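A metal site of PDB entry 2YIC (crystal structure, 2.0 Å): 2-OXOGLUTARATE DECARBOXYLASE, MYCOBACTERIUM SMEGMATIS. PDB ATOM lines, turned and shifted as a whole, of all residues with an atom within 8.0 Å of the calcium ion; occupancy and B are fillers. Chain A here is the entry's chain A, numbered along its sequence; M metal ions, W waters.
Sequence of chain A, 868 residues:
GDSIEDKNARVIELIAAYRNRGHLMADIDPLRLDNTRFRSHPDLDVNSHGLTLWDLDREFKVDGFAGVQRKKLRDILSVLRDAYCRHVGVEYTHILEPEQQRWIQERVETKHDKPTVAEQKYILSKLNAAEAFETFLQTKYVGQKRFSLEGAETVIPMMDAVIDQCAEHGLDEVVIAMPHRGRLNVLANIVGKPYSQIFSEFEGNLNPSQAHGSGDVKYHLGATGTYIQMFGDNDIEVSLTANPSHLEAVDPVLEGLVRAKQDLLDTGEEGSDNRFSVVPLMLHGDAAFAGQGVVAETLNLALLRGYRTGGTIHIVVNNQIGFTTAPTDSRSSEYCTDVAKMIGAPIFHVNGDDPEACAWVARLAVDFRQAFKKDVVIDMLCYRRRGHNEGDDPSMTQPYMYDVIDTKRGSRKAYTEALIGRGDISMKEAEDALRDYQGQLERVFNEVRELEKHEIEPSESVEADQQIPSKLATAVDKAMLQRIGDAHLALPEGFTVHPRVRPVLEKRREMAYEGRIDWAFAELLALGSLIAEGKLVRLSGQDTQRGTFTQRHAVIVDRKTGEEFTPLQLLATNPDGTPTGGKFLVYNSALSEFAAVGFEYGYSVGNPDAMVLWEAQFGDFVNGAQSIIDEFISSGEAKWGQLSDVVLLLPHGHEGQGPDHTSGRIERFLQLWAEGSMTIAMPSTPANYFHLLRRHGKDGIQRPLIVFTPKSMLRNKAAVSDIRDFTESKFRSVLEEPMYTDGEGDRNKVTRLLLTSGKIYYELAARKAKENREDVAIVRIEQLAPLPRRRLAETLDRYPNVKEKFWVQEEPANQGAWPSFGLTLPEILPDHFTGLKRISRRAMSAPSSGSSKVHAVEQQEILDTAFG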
ATOM      1  N   LYS A 535      23.423 -14.355  23.432  1.00  0.00           N
ATOM      2  CA  LYS A 535      22.402 -13.341  23.200  1.00  0.00           C
ATOM      3  C   LYS A 535      22.981 -11.940  23.018  1.00  0.00           C
ATOM      4  O   LYS A 535      23.930 -11.545  23.697  1.00  0.00           O
ATOM      5  CB  LYS A 535      21.374 -13.309  24.353  1.00  0.00           C
ATOM      6  CG  LYS A 535      19.996 -12.831  23.897  1.00  0.00           C
ATOM      7  CD  LYS A 535      18.915 -13.182  24.877  1.00  0.00           C
ATOM      8  CE  LYS A 535      17.559 -12.750  24.377  1.00  0.00           C
ATOM      9  NZ  LYS A 535      17.019 -13.690  23.376  1.00  0.00           N
ATOM     10  N   PRO A 608      13.983  -9.674  17.030  1.00  0.00           N
ATOM     11  CA  PRO A 608      13.269 -10.369  18.118  1.00  0.00           C
ATOM     12  C   PRO A 608      14.172 -11.235  19.023  1.00  0.00           C
ATOM     13  O   PRO A 608      13.744 -11.596  20.114  1.00  0.00           O
ATOM     14  CB  PRO A 608      12.244 -11.242  17.382  1.00  0.00           C
ATOM     15  CG  PRO A 608      12.173 -10.697  15.992  1.00  0.00           C
ATOM     16  CD  PRO A 608      13.506 -10.092  15.702  1.00  0.00           C
ATOM     17  N   ALA A 610      17.033 -10.249  20.321  1.00  0.00           N
ATOM     18  CA  ALA A 610      17.816  -9.385  21.187  1.00  0.00           C
ATOM     19  C   ALA A 610      17.112  -9.208  22.521  1.00  0.00           C
ATOM     20  O   ALA A 610      15.879  -9.232  22.598  1.00  0.00           O
ATOM     21  CB  ALA A 610      17.989  -8.030  20.522  1.00  0.00           C
ATOM     22  N   MET A 611      17.910  -9.020  23.570  1.00  0.00           N
ATOM     23  CA  MET A 611      17.431  -8.634  24.895  1.00  0.00           C
ATOM     24  C   MET A 611      17.534  -7.082  24.895  1.00  0.00           C
ATOM     25  O   MET A 611      18.629  -6.571  24.788  1.00  0.00           O
ATOM     26  CB  MET A 611      18.293  -9.301  25.997  1.00  0.00           C
ATOM     27  CG  MET A 611      17.876  -8.928  27.420  1.00  0.00           C
ATOM     28  SD  MET A 611      16.490  -9.896  28.049  1.00  0.00           S
ATOM     29  CE  MET A 611      16.478  -9.325  29.699  1.00  0.00           C
ATOM     30  N   SER A 644       6.830  -7.416  20.317  1.00  0.00           N
ATOM     31  CA  SER A 644       7.992  -6.788  20.940  1.00  0.00           C
ATOM     32  C   SER A 644       8.306  -7.487  22.269  1.00  0.00           C
ATOM     33  O   SER A 644       7.388  -7.768  23.029  1.00  0.00           O
ATOM     34  CB  SER A 644       7.707  -5.308  21.208  1.00  0.00           C
ATOM     35  OG  SER A 644       8.863  -4.644  21.702  1.00  0.00           O
ATOM     36  N   ASP A 645       9.588  -7.637  22.591  1.00  0.00           N
ATOM     37  CA  ASP A 645      10.079  -8.192  23.857  1.00  0.00           C
ATOM     38  C   ASP A 645      10.797  -7.104  24.671  1.00  0.00           C
ATOM     39  O   ASP A 645      11.598  -7.427  25.553  1.00  0.00           O
ATOM     40  CB  ASP A 645      11.027  -9.368  23.564  1.00  0.00           C
ATOM     41  CG  ASP A 645      10.954 -10.499  24.587  1.00  0.00           C
ATOM     42  OD1 ASP A 645       9.850 -10.741  25.135  1.00  0.00           O
ATOM     43  OD2 ASP A 645      11.996 -11.108  24.860  1.00  0.00           O
ATOM     44  N   VAL A 646      10.515  -5.825  24.369  1.00  0.00           N
ATOM     45  CA  VAL A 646      11.200  -4.688  25.040  1.00  0.00           C
ATOM     46  C   VAL A 646      10.980  -4.726  26.566  1.00  0.00           C
ATOM     47  O   VAL A 646       9.901  -5.080  27.017  1.00  0.00           O
ATOM     48  CB  VAL A 646      10.800  -3.303  24.433  1.00  0.00           C
ATOM     49  CG1 VAL A 646       9.351  -2.904  24.769  1.00  0.00           C
ATOM     50  CG2 VAL A 646      11.770  -2.196  24.888  1.00  0.00           C
ATOM     51  N   VAL A 647      12.009  -4.353  27.320  1.00  0.00           N
ATOM     52  CA  VAL A 647      11.962  -4.235  28.788  1.00  0.00           C
ATOM     53  C   VAL A 647      12.026  -2.763  29.185  1.00  0.00           C
ATOM     54  O   VAL A 647      12.945  -2.060  28.770  1.00  0.00           O
ATOM     55  CB  VAL A 647      13.086  -5.021  29.529  1.00  0.00           C
ATOM     56  CG1 VAL A 647      12.876  -4.958  31.048  1.00  0.00           C
ATOM     57  CG2 VAL A 647      13.162  -6.467  29.060  1.00  0.00           C
ATOM     58  N   THR A 679       4.035  -8.433  30.728  1.00  0.00           N
ATOM     59  CA  THR A 679       4.391  -8.981  32.029  1.00  0.00           C
ATOM     60  C   THR A 679       4.768  -7.770  32.850  1.00  0.00           C
ATOM     61  O   THR A 679       5.510  -6.907  32.357  1.00  0.00           O
ATOM     62  CB  THR A 679       5.519 -10.039  31.932  1.00  0.00           C
ATOM     63  OG1 THR A 679       5.167 -10.989  30.941  1.00  0.00           O
ATOM     64  CG2 THR A 679       5.766 -10.751  33.278  1.00  0.00           C
ATOM     65  N   LEU A 692      13.923 -13.268  36.625  1.00  0.00           N
ATOM     66  CA  LEU A 692      12.920 -12.573  35.830  1.00  0.00           C
ATOM     67  C   LEU A 692      13.486 -12.165  34.439  1.00  0.00           C
ATOM     68  O   LEU A 692      12.864 -12.448  33.426  1.00  0.00           O
ATOM     69  CB  LEU A 692      12.418 -11.325  36.574  1.00  0.00           C
ATOM     70  CG  LEU A 692      11.367 -10.451  35.829  1.00  0.00           C
ATOM     71  CD1 LEU A 692       9.970 -11.031  35.933  1.00  0.00           C
ATOM     72  CD2 LEU A 692      11.342  -9.060  36.390  1.00  0.00           C
ATOM     73  N   LEU A 693      14.697 -11.595  34.430  1.00  0.00           N
ATOM     74  CA  LEU A 693      15.359 -11.163  33.191  1.00  0.00           C
ATOM     75  C   LEU A 693      15.782 -12.340  32.311  1.00  0.00           C
ATOM     76  O   LEU A 693      15.594 -12.285  31.095  1.00  0.00           O
ATOM     77  CB  LEU A 693      16.586 -10.277  33.487  1.00  0.00           C
ATOM     78  CG  LEU A 693      16.357  -8.903  34.133  1.00  0.00           C
ATOM     79  CD1 LEU A 693      17.674  -8.211  34.407  1.00  0.00           C
ATOM     80  CD2 LEU A 693      15.469  -8.019  33.273  1.00  0.00           C
ATOM     81  N   ARG A 694      16.326 -13.401  32.917  1.00  0.00           N
ATOM     82  CA  ARG A 694      16.763 -14.578  32.144  1.00  0.00           C
ATOM     83  C   ARG A 694      15.541 -15.314  31.585  1.00  0.00           C
ATOM     84  O   ARG A 694      15.582 -15.718  30.435  1.00  0.00           O
ATOM     85  CB  ARG A 694      17.650 -15.493  33.003  1.00  0.00           C
ATOM     86  CG  ARG A 694      19.054 -14.922  33.154  1.00  0.00           C
ATOM     87  CD  ARG A 694      20.065 -15.874  33.788  1.00  0.00           C
ATOM     88  NE  ARG A 694      20.010 -17.247  33.276  1.00  0.00           N
ATOM     89  CZ  ARG A 694      20.585 -17.682  32.160  1.00  0.00           C
ATOM     90  NH1 ARG A 694      21.277 -16.860  31.383  1.00  0.00           N
ATOM     91  NH2 ARG A 694      20.443 -18.940  31.787  1.00  0.00           N
ATOM     92  N   ARG A 695      14.434 -15.390  32.362  1.00  0.00           N
ATOM     93  CA  ARG A 695      13.196 -16.026  31.857  1.00  0.00           C
ATOM     94  C   ARG A 695      12.696 -15.226  30.645  1.00  0.00           C
ATOM     95  O   ARG A 695      12.381 -15.802  29.626  1.00  0.00           O
ATOM     96  CB  ARG A 695      12.115 -16.083  32.975  1.00  0.00           C
ATOM     97  CG  ARG A 695      10.797 -16.744  32.564  1.00  0.00           C
ATOM     98  CD  ARG A 695       9.755 -16.704  33.687  1.00  0.00           C
ATOM     99  NE  ARG A 695       9.232 -15.348  33.905  1.00  0.00           N
ATOM    100  CZ  ARG A 695       8.134 -15.035  34.596  1.00  0.00           C
ATOM    101  NH1 ARG A 695       7.410 -15.992  35.156  1.00  0.00           N
ATOM    102  NH2 ARG A 695       7.758 -13.773  34.729  1.00  0.00           N
ATOM    103  N   HIS A 696      12.672 -13.891  30.767  1.00  0.00           N
ATOM    104  CA  HIS A 696      12.221 -12.968  29.735  1.00  0.00           C
ATOM    105  C   HIS A 696      13.005 -13.154  28.445  1.00  0.00           C
ATOM    106  O   HIS A 696      12.410 -13.163  27.367  1.00  0.00           O
ATOM    107  CB  HIS A 696      12.338 -11.510  30.224  1.00  0.00           C
ATOM    108  CG  HIS A 696      11.893 -10.533  29.202  1.00  0.00           C
ATOM    109  ND1 HIS A 696      10.553 -10.311  28.953  1.00  0.00           N
ATOM    110  CD2 HIS A 696      12.614  -9.778  28.342  1.00  0.00           C
ATOM    111  CE1 HIS A 696      10.501  -9.430  27.957  1.00  0.00           C
ATOM    112  NE2 HIS A 696      11.720  -9.086  27.557  1.00  0.00           N
ATOM    113  N   GLY A 697      14.317 -13.275  28.548  1.00  0.00           N
ATOM    114  CA  GLY A 697      15.159 -13.437  27.376  1.00  0.00           C
ATOM    115  C   GLY A 697      15.190 -14.828  26.778  1.00  0.00           C
ATOM    116  O   GLY A 697      15.546 -14.980  25.623  1.00  0.00           O
ATOM    117  N   LYS A 698      14.826 -15.861  27.560  1.00  0.00           N
ATOM    118  CA  LYS A 698      14.931 -17.251  27.091  1.00  0.00           C
ATOM    119  C   LYS A 698      13.583 -17.953  26.837  1.00  0.00           C
ATOM    120  O   LYS A 698      13.590 -19.077  26.326  1.00  0.00           O
ATOM    121  CB  LYS A 698      15.701 -18.072  28.155  1.00  0.00           C
ATOM    122  CG  LYS A 698      17.157 -17.658  28.360  1.00  0.00           C
ATOM    123  CD  LYS A 698      17.787 -18.350  29.580  1.00  0.00           C
ATOM    124  CE  LYS A 698      18.067 -19.835  29.379  1.00  0.00           C
ATOM    125  NZ  LYS A 698      19.074 -20.059  28.288  1.00  0.00           N
ATOM    126  N   ASP A 699      12.437 -17.335  27.197  1.00  0.00           N
ATOM    127  CA  ASP A 699      11.112 -17.961  27.121  1.00  0.00           C
ATOM    128  C   ASP A 699      10.541 -18.169  25.696  1.00  0.00           C
ATOM    129  O   ASP A 699       9.490 -18.798  25.560  1.00  0.00           O
ATOM    130  CB  ASP A 699      10.104 -17.208  27.991  1.00  0.00           C
ATOM    131  CG  ASP A 699       9.867 -15.736  27.660  1.00  0.00           C
ATOM    132  OD1 ASP A 699      10.343 -15.276  26.595  1.00  0.00           O
ATOM    133  OD2 ASP A 699       9.168 -15.065  28.439  1.00  0.00           O
ATOM    134  N   GLY A 700      11.202 -17.649  24.663  1.00  0.00           N
ATOM    135  CA  GLY A 700      10.757 -17.765  23.264  1.00  0.00           C
ATOM    136  C   GLY A 700       9.428 -17.097  22.960  1.00  0.00           C
ATOM    137  O   GLY A 700       8.763 -17.446  21.980  1.00  0.00           O
ATOM    138  N   ILE A 701       9.041 -16.118  23.789  1.00  0.00           N
ATOM    139  CA  ILE A 701       7.795 -15.357  23.748  1.00  0.00           C
ATOM    140  C   ILE A 701       8.180 -13.880  23.659  1.00  0.00           C
ATOM    141  O   ILE A 701       8.995 -13.407  24.453  1.00  0.00           O
ATOM    142  CB  ILE A 701       6.974 -15.709  25.040  1.00  0.00           C
ATOM    143  CG1 ILE A 701       6.306 -17.121  24.894  1.00  0.00           C
ATOM    144  CG2 ILE A 701       5.948 -14.631  25.419  1.00  0.00           C
ATOM    145  CD1 ILE A 701       6.263 -17.945  26.142  1.00  0.00           C
ATOM    146  N   GLN A 702       7.659 -13.180  22.635  1.00  0.00           N
ATOM    147  CA  GLN A 702       7.900 -11.757  22.435  1.00  0.00           C
ATOM    148  C   GLN A 702       6.783 -11.017  23.138  1.00  0.00           C
ATOM    149  O   GLN A 702       5.676 -10.909  22.624  1.00  0.00           O
ATOM    150  CB  GLN A 702       7.978 -11.414  20.952  1.00  0.00           C
ATOM    151  CG  GLN A 702       8.952 -12.281  20.101  1.00  0.00           C
ATOM    152  CD  GLN A 702      10.310 -12.409  20.737  1.00  0.00           C
ATOM    153  OE1 GLN A 702      11.046 -11.434  20.875  1.00  0.00           O
ATOM    154  NE2 GLN A 702      10.646 -13.620  21.164  1.00  0.00           N
ATOM    155  N   ARG A 703       7.046 -10.554  24.352  1.00  0.00           N
ATOM    156  CA  ARG A 703       6.041  -9.853  25.137  1.00  0.00           C
ATOM    157  C   ARG A 703       6.742  -8.816  25.984  1.00  0.00           C
ATOM    158  O   ARG A 703       7.667  -9.184  26.701  1.00  0.00           O
ATOM    159  CB  ARG A 703       5.249 -10.841  26.008  1.00  0.00           C
ATOM    160  CG  ARG A 703       4.094 -10.227  26.813  1.00  0.00           C
ATOM    161  CD  ARG A 703       3.231 -11.274  27.486  1.00  0.00           C
ATOM    162  NE  ARG A 703       2.675 -12.231  26.534  1.00  0.00           N
ATOM    163  CZ  ARG A 703       2.265 -13.452  26.851  1.00  0.00           C
ATOM    164  NH1 ARG A 703       2.317 -13.863  28.116  1.00  0.00           N
ATOM    165  NH2 ARG A 703       1.771 -14.249  25.925  1.00  0.00           N
ATOM    166  N   PRO A 704       6.283  -7.538  26.014  1.00  0.00           N
ATOM    167  CA  PRO A 704       6.997  -6.526  26.815  1.00  0.00           C
ATOM    168  C   PRO A 704       6.963  -6.838  28.294  1.00  0.00           C
ATOM    169  O   PRO A 704       6.024  -7.460  28.769  1.00  0.00           O
ATOM    170  CB  PRO A 704       6.222  -5.236  26.522  1.00  0.00           C
ATOM    171  CG  PRO A 704       5.613  -5.465  25.156  1.00  0.00           C
ATOM    172  CD  PRO A 704       5.184  -6.913  25.237  1.00  0.00           C
ATOM    173  N   LEU A 705       8.035  -6.448  28.982  1.00  0.00           N
ATOM    174  CA  LEU A 705       8.196  -6.635  30.423  1.00  0.00           C
ATOM    175  C   LEU A 705       8.395  -5.275  31.074  1.00  0.00           C
ATOM    176  O   LEU A 705       9.270  -4.485  30.668  1.00  0.00           O
ATOM    177  CB  LEU A 705       9.359  -7.599  30.738  1.00  0.00           C
ATOM    178  CG  LEU A 705       9.785  -7.700  32.226  1.00  0.00           C
ATOM    179  CD1 LEU A 705       8.706  -8.395  33.079  1.00  0.00           C
ATOM    180  CD2 LEU A 705      11.131  -8.377  32.370  1.00  0.00           C
HETATM  181 CA    CA M   1      10.712 -13.031  25.833  1.00  0.00          CA
HETATM  182  O   HOH W   1      12.101 -14.185  24.218  1.00  0.00           O
HETATM  183  O   HOH W   2       9.150 -12.650  27.339  1.00  0.00           O
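The side-chain carboxylate of Asp 645 lies close to the backbone NH of Arg 703.
Of the 23 residues printed, 4 come within 4 Å of the calcium ion.
Along chain A the residues within 4 Å of the calcium ion span positions 645 to 701.
Water W2 bridges OD2 of Asp 699 and ND1 of His 696.
Water W2 binds the calcium ion.
The calcium ion is bound by the backbone carbonyl oxygen (O) of Ile 701, at 2.2 Å.
The backbone carbonyl oxygen (O) of His 696 binds the calcium ion, 2.3 Å away.
OD1 of Asp 699 is bound to the calcium ion (2.4 Å).
The calcium ion is bound by water W1, at 2.4 Å.
The calcium ion is bound by the side-chain carboxylate (OD2) of Asp 645, at 2.5 Å.
The calcium ion is bound by OD1 of Asp 645 (2.5 Å).
The calcium ion has seven donor atoms within binding distance.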
